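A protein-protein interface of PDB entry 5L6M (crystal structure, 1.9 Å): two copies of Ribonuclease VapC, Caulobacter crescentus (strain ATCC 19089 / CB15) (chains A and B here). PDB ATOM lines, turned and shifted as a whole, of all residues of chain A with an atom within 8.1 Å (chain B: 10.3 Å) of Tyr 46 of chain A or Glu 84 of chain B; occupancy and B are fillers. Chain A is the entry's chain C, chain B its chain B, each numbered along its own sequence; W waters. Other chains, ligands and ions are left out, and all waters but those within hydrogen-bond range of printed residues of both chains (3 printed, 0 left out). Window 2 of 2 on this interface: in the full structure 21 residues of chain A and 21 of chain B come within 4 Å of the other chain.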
ATOM      1  N   ARG A  14      14.532  -1.205   0.751  1.00  0.00           N
ATOM      2  CA  ARG A  14      14.646  -1.945  -0.501  1.00  0.00           C
ATOM      3  C   ARG A  14      13.474  -1.647  -1.436  1.00  0.00           C
ATOM      4  O   ARG A  14      13.661  -1.508  -2.645  1.00  0.00           O
ATOM      5  CB  ARG A  14      14.711  -3.460  -0.247  1.00  0.00           C
ATOM      6  CG  ARG A  14      14.960  -4.265  -1.526  1.00  0.00           C
ATOM      7  CD  ARG A  14      14.574  -5.760  -1.379  1.00  0.00           C
ATOM      8  NE  ARG A  14      13.175  -5.908  -0.945  1.00  0.00           N
ATOM      9  CZ  ARG A  14      12.682  -6.961  -0.298  1.00  0.00           C
ATOM     10  NH1 ARG A  14      13.459  -8.000  -0.017  1.00  0.00           N
ATOM     11  NH2 ARG A  14      11.400  -6.982   0.052  1.00  0.00           N
ATOM     12  N   LEU A  41      15.676 -10.465   4.198  1.00  0.00           N
ATOM     13  CA  LEU A  41      15.545  -9.750   2.934  1.00  0.00           C
ATOM     14  C   LEU A  41      15.742 -10.668   1.724  1.00  0.00           C
ATOM     15  O   LEU A  41      15.100 -10.473   0.683  1.00  0.00           O
ATOM     16  CB  LEU A  41      16.551  -8.603   2.888  1.00  0.00           C
ATOM     17  CG  LEU A  41      16.300  -7.454   3.854  1.00  0.00           C
ATOM     18  CD1 LEU A  41      17.611  -6.695   4.016  1.00  0.00           C
ATOM     19  CD2 LEU A  41      15.271  -6.569   3.223  1.00  0.00           C
ATOM     20  N   GLU A  42      16.645 -11.650   1.826  1.00  0.00           N
ATOM     21  CA  GLU A  42      16.908 -12.518   0.679  1.00  0.00           C
ATOM     22  C   GLU A  42      15.697 -13.386   0.388  1.00  0.00           C
ATOM     23  O   GLU A  42      15.379 -13.644  -0.778  1.00  0.00           O
ATOM     24  CB  GLU A  42      18.142 -13.420   0.904  1.00  0.00           C
ATOM     25  CG  GLU A  42      19.502 -12.701   1.073  1.00  0.00           C
ATOM     26  CD  GLU A  42      20.176 -12.330  -0.249  1.00  0.00           C
ATOM     27  OE1 GLU A  42      19.535 -12.515  -1.314  1.00  0.00           O
ATOM     28  OE2 GLU A  42      21.339 -11.852  -0.198  1.00  0.00           O
ATOM     29  N   GLY A  43      14.989 -13.808   1.444  1.00  0.00           N
ATOM     30  CA  GLY A  43      13.787 -14.612   1.297  1.00  0.00           C
ATOM     31  C   GLY A  43      12.633 -13.893   0.627  1.00  0.00           C
ATOM     32  O   GLY A  43      11.735 -14.555   0.106  1.00  0.00           O
ATOM     33  N   GLY A  44      12.618 -12.552   0.649  1.00  0.00           N
ATOM     34  CA  GLY A  44      11.521 -11.840   0.027  1.00  0.00           C
ATOM     35  C   GLY A  44      11.705 -11.500  -1.439  1.00  0.00           C
ATOM     36  O   GLY A  44      10.760 -11.014  -2.083  1.00  0.00           O
ATOM     37  N   VAL A  45      12.906 -11.733  -1.982  1.00  0.00           N
ATOM     38  CA  VAL A  45      13.220 -11.286  -3.337  1.00  0.00           C
ATOM     39  C   VAL A  45      12.295 -11.929  -4.359  1.00  0.00           C
ATOM     40  O   VAL A  45      11.837 -11.268  -5.293  1.00  0.00           O
ATOM     41  CB  VAL A  45      14.690 -11.575  -3.675  1.00  0.00           C
ATOM     42  CG1 VAL A  45      14.923 -11.412  -5.190  1.00  0.00           C
ATOM     43  CG2 VAL A  45      15.577 -10.649  -2.888  1.00  0.00           C
ATOM     44  N   TYR A  46      12.029 -13.228  -4.229  1.00  0.00           N
ATOM     45  CA  TYR A  46      11.251 -13.933  -5.248  1.00  0.00           C
ATOM     46  C   TYR A  46       9.816 -14.183  -4.811  1.00  0.00           C
ATOM     47  O   TYR A  46       9.114 -14.991  -5.435  1.00  0.00           O
ATOM     48  CB  TYR A  46      11.944 -15.246  -5.646  1.00  0.00           C
ATOM     49  CG  TYR A  46      13.396 -15.047  -6.021  1.00  0.00           C
ATOM     50  CD1 TYR A  46      13.771 -14.764  -7.335  1.00  0.00           C
ATOM     51  CD2 TYR A  46      14.392 -15.089  -5.054  1.00  0.00           C
ATOM     52  CE1 TYR A  46      15.108 -14.548  -7.674  1.00  0.00           C
ATOM     53  CE2 TYR A  46      15.723 -14.883  -5.378  1.00  0.00           C
ATOM     54  CZ  TYR A  46      16.083 -14.610  -6.699  1.00  0.00           C
ATOM     55  OH  TYR A  46      17.427 -14.413  -7.007  1.00  0.00           O
ATOM     56  N   ARG A  47       9.369 -13.490  -3.759  1.00  0.00           N
ATOM     57  CA  ARG A  47       7.985 -13.601  -3.293  1.00  0.00           C
ATOM     58  C   ARG A  47       7.002 -13.350  -4.430  1.00  0.00           C
ATOM     59  O   ARG A  47       6.134 -14.181  -4.714  1.00  0.00           O
ATOM     60  CB  ARG A  47       7.757 -12.611  -2.143  1.00  0.00           C
ATOM     61  CG  ARG A  47       6.311 -12.341  -1.740  1.00  0.00           C
ATOM     62  CD  ARG A  47       5.911 -13.129  -0.495  1.00  0.00           C
ATOM     63  NE  ARG A  47       6.912 -13.101   0.581  1.00  0.00           N
ATOM     64  CZ  ARG A  47       6.894 -12.261   1.616  1.00  0.00           C
ATOM     65  NH1 ARG A  47       5.931 -11.352   1.729  1.00  0.00           N
ATOM     66  NH2 ARG A  47       7.844 -12.328   2.541  1.00  0.00           N
ATOM     67  N   GLU A  48       7.137 -12.213  -5.102  1.00  0.00           N
ATOM     68  CA  GLU A  48       6.259 -11.818  -6.199  1.00  0.00           C
ATOM     69  C   GLU A  48       7.067 -11.938  -7.488  1.00  0.00           C
ATOM     70  O   GLU A  48       7.965 -11.123  -7.741  1.00  0.00           O
ATOM     71  CB  GLU A  48       5.736 -10.396  -5.985  1.00  0.00           C
ATOM     72  CG  GLU A  48       4.991 -10.206  -4.658  1.00  0.00           C
ATOM     73  CD  GLU A  48       4.851  -8.741  -4.250  1.00  0.00           C
ATOM     74  OE1 GLU A  48       4.493  -8.478  -3.077  1.00  0.00           O
ATOM     75  OE2 GLU A  48       5.107  -7.855  -5.098  1.00  0.00           O
ATOM     76  N   ALA A  49       6.747 -12.955  -8.294  1.00  0.00           N
ATOM     77  CA  ALA A  49       7.625 -13.360  -9.387  1.00  0.00           C
ATOM     78  C   ALA A  49       7.926 -12.198 -10.323  1.00  0.00           C
ATOM     79  O   ALA A  49       9.077 -11.984 -10.708  1.00  0.00           O
ATOM     80  CB  ALA A  49       6.995 -14.516 -10.173  1.00  0.00           C
ATOM     81  N   ALA A  50       6.899 -11.429 -10.687  1.00  0.00           N
ATOM     82  CA  ALA A  50       7.068 -10.352 -11.659  1.00  0.00           C
ATOM     83  C   ALA A  50       7.960  -9.231 -11.146  1.00  0.00           C
ATOM     84  O   ALA A  50       8.479  -8.459 -11.951  1.00  0.00           O
ATOM     85  CB  ALA A  50       5.707  -9.790 -12.056  1.00  0.00           C
ATOM     86  N   GLN A  51       8.155  -9.130  -9.838  1.00  0.00           N
ATOM     87  CA  GLN A  51       9.002  -8.117  -9.211  1.00  0.00           C
ATOM     88  C   GLN A  51      10.377  -8.657  -8.820  1.00  0.00           C
ATOM     89  O   GLN A  51      11.183  -7.924  -8.219  1.00  0.00           O
ATOM     90  CB  GLN A  51       8.299  -7.572  -7.962  1.00  0.00           C
ATOM     91  CG  GLN A  51       6.872  -7.080  -8.218  1.00  0.00           C
ATOM     92  CD  GLN A  51       6.860  -5.772  -8.953  1.00  0.00           C
ATOM     93  OE1 GLN A  51       7.461  -4.803  -8.506  1.00  0.00           O
ATOM     94  NE2 GLN A  51       6.186  -5.733 -10.094  1.00  0.00           N
ATOM     95  N   ALA A  52      10.647  -9.927  -9.121  1.00  0.00           N
ATOM     96  CA  ALA A  52      11.856 -10.582  -8.631  1.00  0.00           C
ATOM     97  C   ALA A  52      13.121  -9.863  -9.102  1.00  0.00           C
ATOM     98  O   ALA A  52      14.044  -9.628  -8.315  1.00  0.00           O
ATOM     99  CB  ALA A  52      11.865 -12.041  -9.096  1.00  0.00           C
ATOM    100  N   GLY A  53      13.201  -9.546 -10.398  1.00  0.00           N
ATOM    101  CA  GLY A  53      14.414  -8.920 -10.904  1.00  0.00           C
ATOM    102  C   GLY A  53      14.651  -7.569 -10.262  1.00  0.00           C
ATOM    103  O   GLY A  53      15.795  -7.187  -9.977  1.00  0.00           O
ATOM    104  N   ARG A  55      13.545  -6.528  -7.150  1.00  0.00           N
ATOM    105  CA  ARG A  55      13.978  -6.696  -5.764  1.00  0.00           C
ATOM    106  C   ARG A  55      15.408  -7.226  -5.686  1.00  0.00           C
ATOM    107  O   ARG A  55      16.180  -6.792  -4.826  1.00  0.00           O
ATOM    108  CB  ARG A  55      13.010  -7.609  -5.006  1.00  0.00           C
ATOM    109  CG  ARG A  55      11.664  -6.920  -4.723  1.00  0.00           C
ATOM    110  CD  ARG A  55      10.911  -7.533  -3.552  1.00  0.00           C
ATOM    111  NE  ARG A  55       9.810  -6.653  -3.130  1.00  0.00           N
ATOM    112  CZ  ARG A  55       8.556  -6.720  -3.586  1.00  0.00           C
ATOM    113  NH1 ARG A  55       7.633  -5.881  -3.125  1.00  0.00           N
ATOM    114  NH2 ARG A  55       8.208  -7.643  -4.473  1.00  0.00           N
ATOM    115  N   ARG A  56      15.773  -8.148  -6.580  1.00  0.00           N
ATOM    116  CA  ARG A  56      17.153  -8.626  -6.694  1.00  0.00           C
ATOM    117  C   ARG A  56      18.115  -7.456  -6.854  1.00  0.00           C
ATOM    118  O   ARG A  56      19.073  -7.293  -6.089  1.00  0.00           O
ATOM    119  CB  ARG A  56      17.280  -9.567  -7.895  1.00  0.00           C
ATOM    120  CG  ARG A  56      18.703 -10.055  -8.219  1.00  0.00           C
ATOM    121  CD  ARG A  56      19.143 -11.231  -7.295  1.00  0.00           C
ATOM    122  NE  ARG A  56      19.607 -10.726  -6.017  1.00  0.00           N
ATOM    123  CZ  ARG A  56      19.318 -11.266  -4.831  1.00  0.00           C
ATOM    124  NH1 ARG A  56      18.563 -12.367  -4.727  1.00  0.00           N
ATOM    125  NH2 ARG A  56      19.808 -10.714  -3.743  1.00  0.00           N
ATOM    126  N   SER A  57      17.861  -6.627  -7.859  1.00  0.00           N
ATOM    127  CA  SER A  57      18.765  -5.523  -8.140  1.00  0.00           C
ATOM    128  C   SER A  57      18.816  -4.546  -6.969  1.00  0.00           C
ATOM    129  O   SER A  57      19.889  -4.065  -6.599  1.00  0.00           O
ATOM    130  CB  SER A  57      18.332  -4.799  -9.417  1.00  0.00           C
ATOM    131  OG  SER A  57      19.492  -4.218 -10.009  1.00  0.00           O
ATOM    132  N   LEU A  59      18.069  -5.005  -3.722  1.00  0.00           N
ATOM    133  CA  LEU A  59      18.771  -5.570  -2.569  1.00  0.00           C
ATOM    134  C   LEU A  59      20.265  -5.658  -2.827  1.00  0.00           C
ATOM    135  O   LEU A  59      21.051  -5.354  -1.924  1.00  0.00           O
ATOM    136  CB  LEU A  59      18.209  -6.951  -2.181  1.00  0.00           C
ATOM    137  CG  LEU A  59      18.955  -7.672  -1.045  1.00  0.00           C
ATOM    138  CD1 LEU A  59      18.931  -6.843   0.280  1.00  0.00           C
ATOM    139  CD2 LEU A  59      18.288  -9.117  -0.823  1.00  0.00           C
ATOM    140  N   ASP A  60      20.679  -6.078  -4.041  1.00  0.00           N
ATOM    141  CA  ASP A  60      22.108  -6.161  -4.358  1.00  0.00           C
ATOM    142  C   ASP A  60      22.786  -4.798  -4.225  1.00  0.00           C
ATOM    143  O   ASP A  60      23.921  -4.703  -3.745  1.00  0.00           O
ATOM    144  CB  ASP A  60      22.344  -6.722  -5.779  1.00  0.00           C
ATOM    145  CG  ASP A  60      21.964  -8.218  -5.891  1.00  0.00           C
ATOM    146  OD1 ASP A  60      21.706  -8.862  -4.830  1.00  0.00           O
ATOM    147  OD2 ASP A  60      21.898  -8.728  -7.033  1.00  0.00           O
ATOM    148  N   ALA B  76      25.066 -16.906   4.386  1.00  0.00           N
ATOM    149  CA  ALA B  76      23.916 -16.212   3.833  1.00  0.00           C
ATOM    150  C   ALA B  76      23.840 -16.380   2.315  1.00  0.00           C
ATOM    151  O   ALA B  76      22.737 -16.397   1.757  1.00  0.00           O
ATOM    152  CB  ALA B  76      24.009 -14.736   4.215  1.00  0.00           C
ATOM    153  N   ASP B  77      24.997 -16.472   1.636  1.00  0.00           N
ATOM    154  CA  ASP B  77      25.009 -16.739   0.195  1.00  0.00           C
ATOM    155  C   ASP B  77      24.371 -18.087  -0.098  1.00  0.00           C
ATOM    156  O   ASP B  77      23.621 -18.239  -1.067  1.00  0.00           O
ATOM    157  CB  ASP B  77      26.432 -16.746  -0.356  1.00  0.00           C
ATOM    158  CG  ASP B  77      27.089 -15.359  -0.380  1.00  0.00           C
ATOM    159  OD1 ASP B  77      26.398 -14.320  -0.278  1.00  0.00           O
ATOM    160  OD2 ASP B  77      28.319 -15.342  -0.513  1.00  0.00           O
ATOM    161  N   GLU B  78      24.707 -19.091   0.709  1.00  0.00           N
ATOM    162  CA  GLU B  78      24.103 -20.401   0.530  1.00  0.00           C
ATOM    163  C   GLU B  78      22.617 -20.356   0.830  1.00  0.00           C
ATOM    164  O   GLU B  78      21.824 -21.043   0.170  1.00  0.00           O
ATOM    165  CB  GLU B  78      24.785 -21.426   1.428  1.00  0.00           C
ATOM    166  CG  GLU B  78      26.205 -21.731   1.041  1.00  0.00           C
ATOM    167  CD  GLU B  78      26.351 -22.562  -0.221  1.00  0.00           C
ATOM    168  OE1 GLU B  78      27.513 -22.921  -0.528  1.00  0.00           O
ATOM    169  OE2 GLU B  78      25.334 -22.872  -0.899  1.00  0.00           O
ATOM    170  N   TYR B  79      22.223 -19.563   1.837  1.00  0.00           N
ATOM    171  CA  TYR B  79      20.805 -19.435   2.147  1.00  0.00           C
ATOM    172  C   TYR B  79      20.060 -18.863   0.951  1.00  0.00           C
ATOM    173  O   TYR B  79      18.998 -19.358   0.564  1.00  0.00           O
ATOM    174  CB  TYR B  79      20.574 -18.550   3.376  1.00  0.00           C
ATOM    175  CG  TYR B  79      19.107 -18.399   3.649  1.00  0.00           C
ATOM    176  CD1 TYR B  79      18.430 -19.326   4.461  1.00  0.00           C
ATOM    177  CD2 TYR B  79      18.368 -17.370   3.062  1.00  0.00           C
ATOM    178  CE1 TYR B  79      17.089 -19.223   4.680  1.00  0.00           C
ATOM    179  CE2 TYR B  79      17.006 -17.273   3.277  1.00  0.00           C
ATOM    180  CZ  TYR B  79      16.375 -18.207   4.092  1.00  0.00           C
ATOM    181  OH  TYR B  79      15.027 -18.111   4.308  1.00  0.00           O
ATOM    182  N   ARG B  80      20.588 -17.784   0.382  1.00  0.00           N
ATOM    183  CA  ARG B  80      19.991 -17.232  -0.831  1.00  0.00           C
ATOM    184  C   ARG B  80      19.817 -18.315  -1.899  1.00  0.00           C
ATOM    185  O   ARG B  80      18.753 -18.435  -2.514  1.00  0.00           O
ATOM    186  CB  ARG B  80      20.873 -16.104  -1.372  1.00  0.00           C
ATOM    187  CG  ARG B  80      20.464 -15.634  -2.767  1.00  0.00           C
ATOM    188  CD  ARG B  80      21.352 -14.510  -3.288  1.00  0.00           C
ATOM    189  NE  ARG B  80      21.241 -14.514  -4.738  1.00  0.00           N
ATOM    190  CZ  ARG B  80      21.826 -13.666  -5.582  1.00  0.00           C
ATOM    191  NH1 ARG B  80      21.608 -13.820  -6.886  1.00  0.00           N
ATOM    192  NH2 ARG B  80      22.642 -12.707  -5.140  1.00  0.00           N
ATOM    193  N   ARG B  81      20.857 -19.126  -2.123  1.00  0.00           N
ATOM    194  CA  ARG B  81      20.733 -20.175  -3.136  1.00  0.00           C
ATOM    195  C   ARG B  81      19.633 -21.165  -2.780  1.00  0.00           C
ATOM    196  O   ARG B  81      18.958 -21.699  -3.669  1.00  0.00           O
ATOM    197  CB  ARG B  81      22.049 -20.927  -3.305  1.00  0.00           C
ATOM    198  CG  ARG B  81      23.103 -20.177  -4.063  1.00  0.00           C
ATOM    199  CD  ARG B  81      24.254 -21.109  -4.432  1.00  0.00           C
ATOM    200  NE  ARG B  81      25.382 -20.931  -3.526  1.00  0.00           N
ATOM    201  CZ  ARG B  81      26.202 -19.885  -3.550  1.00  0.00           C
ATOM    202  NH1 ARG B  81      26.018 -18.917  -4.434  1.00  0.00           N
ATOM    203  NH2 ARG B  81      27.202 -19.808  -2.683  1.00  0.00           N
ATOM    204  N   ILE B  82      19.452 -21.442  -1.493  1.00  0.00           N
ATOM    205  CA  ILE B  82      18.405 -22.380  -1.097  1.00  0.00           C
ATOM    206  C   ILE B  82      17.051 -21.817  -1.504  1.00  0.00           C
ATOM    207  O   ILE B  82      16.245 -22.484  -2.152  1.00  0.00           O
ATOM    208  CB  ILE B  82      18.472 -22.669   0.414  1.00  0.00           C
ATOM    209  CG1 ILE B  82      19.733 -23.486   0.754  1.00  0.00           C
ATOM    210  CG2 ILE B  82      17.239 -23.465   0.891  1.00  0.00           C
ATOM    211  CD1 ILE B  82      19.905 -23.728   2.262  1.00  0.00           C
ATOM    212  N   VAL B  83      16.817 -20.549  -1.173  1.00  0.00           N
ATOM    213  CA  VAL B  83      15.561 -19.912  -1.534  1.00  0.00           C
ATOM    214  C   VAL B  83      15.375 -19.868  -3.060  1.00  0.00           C
ATOM    215  O   VAL B  83      14.262 -20.080  -3.563  1.00  0.00           O
ATOM    216  CB  VAL B  83      15.511 -18.511  -0.913  1.00  0.00           C
ATOM    217  CG1 VAL B  83      14.357 -17.746  -1.540  1.00  0.00           C
ATOM    218  CG2 VAL B  83      15.305 -18.643   0.569  1.00  0.00           C
ATOM    219  N   GLU B  84      16.447 -19.594  -3.820  1.00  0.00           N
ATOM    220  CA  GLU B  84      16.319 -19.565  -5.284  1.00  0.00           C
ATOM    221  C   GLU B  84      15.880 -20.917  -5.832  1.00  0.00           C
ATOM    222  O   GLU B  84      15.060 -20.983  -6.745  1.00  0.00           O
ATOM    223  CB  GLU B  84      17.635 -19.119  -5.941  1.00  0.00           C
ATOM    224  CG  GLU B  84      18.006 -17.668  -5.593  1.00  0.00           C
ATOM    225  CD  GLU B  84      19.389 -17.253  -6.086  1.00  0.00           C
ATOM    226  OE1 GLU B  84      20.277 -18.123  -6.254  1.00  0.00           O
ATOM    227  OE2 GLU B  84      19.588 -16.033  -6.313  1.00  0.00           O
ATOM    228  N   SER B  85      16.401 -22.007  -5.275  1.00  0.00           N
ATOM    229  CA  SER B  85      16.078 -23.336  -5.777  1.00  0.00           C
ATOM    230  C   SER B  85      14.759 -23.860  -5.221  1.00  0.00           C
ATOM    231  O   SER B  85      13.985 -24.493  -5.944  1.00  0.00           O
ATOM    232  CB  SER B  85      17.201 -24.304  -5.414  1.00  0.00           C
ATOM    233  OG  SER B  85      18.212 -24.271  -6.395  1.00  0.00           O
ATOM    234  N   ALA B  86      14.511 -23.682  -3.928  1.00  0.00           N
ATOM    235  CA  ALA B  86      13.387 -24.363  -3.309  1.00  0.00           C
ATOM    236  C   ALA B  86      12.196 -23.455  -3.057  1.00  0.00           C
ATOM    237  O   ALA B  86      11.113 -23.961  -2.727  1.00  0.00           O
ATOM    238  CB  ALA B  86      13.820 -25.022  -1.999  1.00  0.00           C
ATOM    239  N   GLY B  87      12.355 -22.147  -3.229  1.00  0.00           N
ATOM    240  CA  GLY B  87      11.341 -21.204  -2.824  1.00  0.00           C
ATOM    241  C   GLY B  87      11.398 -20.923  -1.332  1.00  0.00           C
ATOM    242  O   GLY B  87      11.904 -21.713  -0.534  1.00  0.00           O
ATOM    243  N   TYR B  88      10.859 -19.767  -0.959  1.00  0.00           N
ATOM    244  CA  TYR B  88      10.858 -19.345   0.437  1.00  0.00           C
ATOM    245  C   TYR B  88       9.925 -20.220   1.278  1.00  0.00           C
ATOM    246  O   TYR B  88       8.893 -20.687   0.794  1.00  0.00           O
ATOM    247  CB  TYR B  88      10.426 -17.875   0.524  1.00  0.00           C
ATOM    248  CG  TYR B  88      10.126 -17.399   1.919  1.00  0.00           C
ATOM    249  CD1 TYR B  88      11.147 -17.194   2.832  1.00  0.00           C
ATOM    250  CD2 TYR B  88       8.820 -17.148   2.317  1.00  0.00           C
ATOM    251  CE1 TYR B  88      10.884 -16.756   4.113  1.00  0.00           C
ATOM    252  CE2 TYR B  88       8.544 -16.713   3.591  1.00  0.00           C
ATOM    253  CZ  TYR B  88       9.583 -16.508   4.485  1.00  0.00           C
ATOM    254  OH  TYR B  88       9.320 -16.081   5.770  1.00  0.00           O
ATOM    255  N   SER B  89      10.308 -20.425   2.548  1.00  0.00           N
ATOM    256  CA  SER B  89       9.525 -21.151   3.553  1.00  0.00           C
ATOM    257  C   SER B  89       9.748 -20.494   4.916  1.00  0.00           C
ATOM    258  O   SER B  89      10.844 -20.587   5.477  1.00  0.00           O
ATOM    259  CB  SER B  89       9.921 -22.631   3.599  1.00  0.00           C
ATOM    260  OG  SER B  89       9.391 -23.263   4.747  1.00  0.00           O
ATOM    261  N   ARG B  96      17.137 -23.789   7.525  1.00  0.00           N
ATOM    262  CA  ARG B  96      17.915 -23.576   6.313  1.00  0.00           C
ATOM    263  C   ARG B  96      19.154 -22.744   6.572  1.00  0.00           C
ATOM    264  O   ARG B  96      20.139 -22.885   5.838  1.00  0.00           O
ATOM    265  CB  ARG B  96      17.053 -22.927   5.244  1.00  0.00           C
ATOM    266  CG  ARG B  96      16.043 -23.879   4.676  1.00  0.00           C
ATOM    267  CD  ARG B  96      15.019 -23.137   3.841  1.00  0.00           C
ATOM    268  NE  ARG B  96      14.228 -24.063   3.027  1.00  0.00           N
ATOM    269  CZ  ARG B  96      13.373 -23.684   2.084  1.00  0.00           C
ATOM    270  NH1 ARG B  96      13.189 -22.399   1.829  1.00  0.00           N
ATOM    271  NH2 ARG B  96      12.716 -24.595   1.394  1.00  0.00           N
ATOM    272  N   ASP B 119      14.942 -30.642   0.271  1.00  0.00           N
ATOM    273  CA  ASP B 119      14.841 -29.713  -0.845  1.00  0.00           C
ATOM    274  C   ASP B 119      16.070 -28.835  -0.978  1.00  0.00           C
ATOM    275  O   ASP B 119      16.046 -27.891  -1.765  1.00  0.00           O
ATOM    276  CB  ASP B 119      13.590 -28.840  -0.721  1.00  0.00           C
ATOM    277  CG  ASP B 119      13.506 -28.088   0.605  1.00  0.00           C
ATOM    278  OD1 ASP B 119      14.462 -28.108   1.414  1.00  0.00           O
ATOM    279  OD2 ASP B 119      12.461 -27.451   0.840  1.00  0.00           O
ATOM    280  N   ILE B 120      17.145 -29.143  -0.256  1.00  0.00           N
ATOM    281  CA  ILE B 120      18.338 -28.307  -0.245  1.00  0.00           C
ATOM    282  C   ILE B 120      19.369 -28.910  -1.193  1.00  0.00           C
ATOM    283  O   ILE B 120      19.991 -29.918  -0.843  1.00  0.00           O
ATOM    284  CB  ILE B 120      18.869 -28.159   1.190  1.00  0.00           C
ATOM    285  CG1 ILE B 120      17.765 -27.567   2.075  1.00  0.00           C
ATOM    286  CG2 ILE B 120      20.178 -27.323   1.247  1.00  0.00           C
ATOM    287  CD1 ILE B 120      18.168 -27.363   3.536  1.00  0.00           C
ATOM    288  N   PRO B 121      19.574 -28.357  -2.400  1.00  0.00           N
ATOM    289  CA  PRO B 121      20.542 -28.970  -3.333  1.00  0.00           C
ATOM    290  C   PRO B 121      21.954 -28.987  -2.760  1.00  0.00           C
ATOM    291  O   PRO B 121      22.414 -28.005  -2.175  1.00  0.00           O
ATOM    292  CB  PRO B 121      20.464 -28.070  -4.579  1.00  0.00           C
ATOM    293  CG  PRO B 121      19.144 -27.421  -4.507  1.00  0.00           C
ATOM    294  CD  PRO B 121      18.848 -27.231  -3.018  1.00  0.00           C
HETATM  295  O   HOH W   1      23.051 -11.048  -6.993  1.00  0.00           O
HETATM  296  O   HOH W   2      22.898 -11.734  -2.263  1.00  0.00           O
HETATM  297  O   HOH W   3      14.367 -15.533   4.371  1.00  0.00           O
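The guanidinium group (NH2) of Arg 80 of chain B lies within salt-bridge range of the side-chain carboxylate (OD1) of Asp 60 of chain A (3.97 Å).
OH of Tyr 46 of chain A sits at hydrogen-bond distance from OE2 of Glu 84 of chain B (2.8 Å).
NH1 of Arg 56 of chain A sits close to NE of Arg 80 of chain B (3.4 Å).
OE2 of Glu 84 of chain B lies within salt-bridge range of NE of Arg 80 of chain B (2.7 Å).
The side-chain carboxylate of Glu 42 of chain A lies within salt-bridge range of the guanidinium group of Arg 56 of chain A, 3.0 Å away.
OH of Tyr 46 of chain A lies within hydrogen-bond range of NH1 of Arg 56 of chain A, at 3.3 Å.
The guanidinium group of Arg 56 of chain A is in salt-bridge range of the side-chain carboxylate of Asp 60 of chain A.
CD of Arg 80 of chain B touches OE1 of Glu 42 of chain A, 3.3 Å away.
Tyr 88 of chain B touches Gly 43 of chain A (CB to O, 3.6 Å).
Of chain B, only Glu 84 comes within 4 Å of Tyr 46 of chain A.
Glu 84 of chain B touches just one residue of chain A: Tyr 46.
No residue of chain B comes within 4 Å of Val 45 of chain A.
Printed residues of chain B within 4 Å of Glu 42 of chain A: Arg 80 (3.3 Å).
Of the printed residues of chain A, Arg 80 of chain B touches Glu 42, Arg 56 and Asp 60.
Arg 81 of chain B touches none of the printed residues of chain A.
The nearest printed residue of chain B that does not touch Glu 42 of chain A is Val 83 of chain B (4.3 Å).
Water W1 bridges the guanidinium group (NH2) of Arg 80 of chain B and the side-chain carboxylate (OD2) of Asp 60 of chain A.
Water W2 lies within hydrogen-bond range of OE2 of Glu 42 of chain A (2.6 Å) and NH2 of Arg 80 of chain B (3.0 Å).
Water W3 bridges the side-chain hydroxyl of Tyr 79 of chain B (2.7 Å) and the backbone NH of Gly 43 of chain A (3.5 Å).
No position is printed for both chains.
Of the 18 printed residues of chain B, 3 touch a printed residue of chain A.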
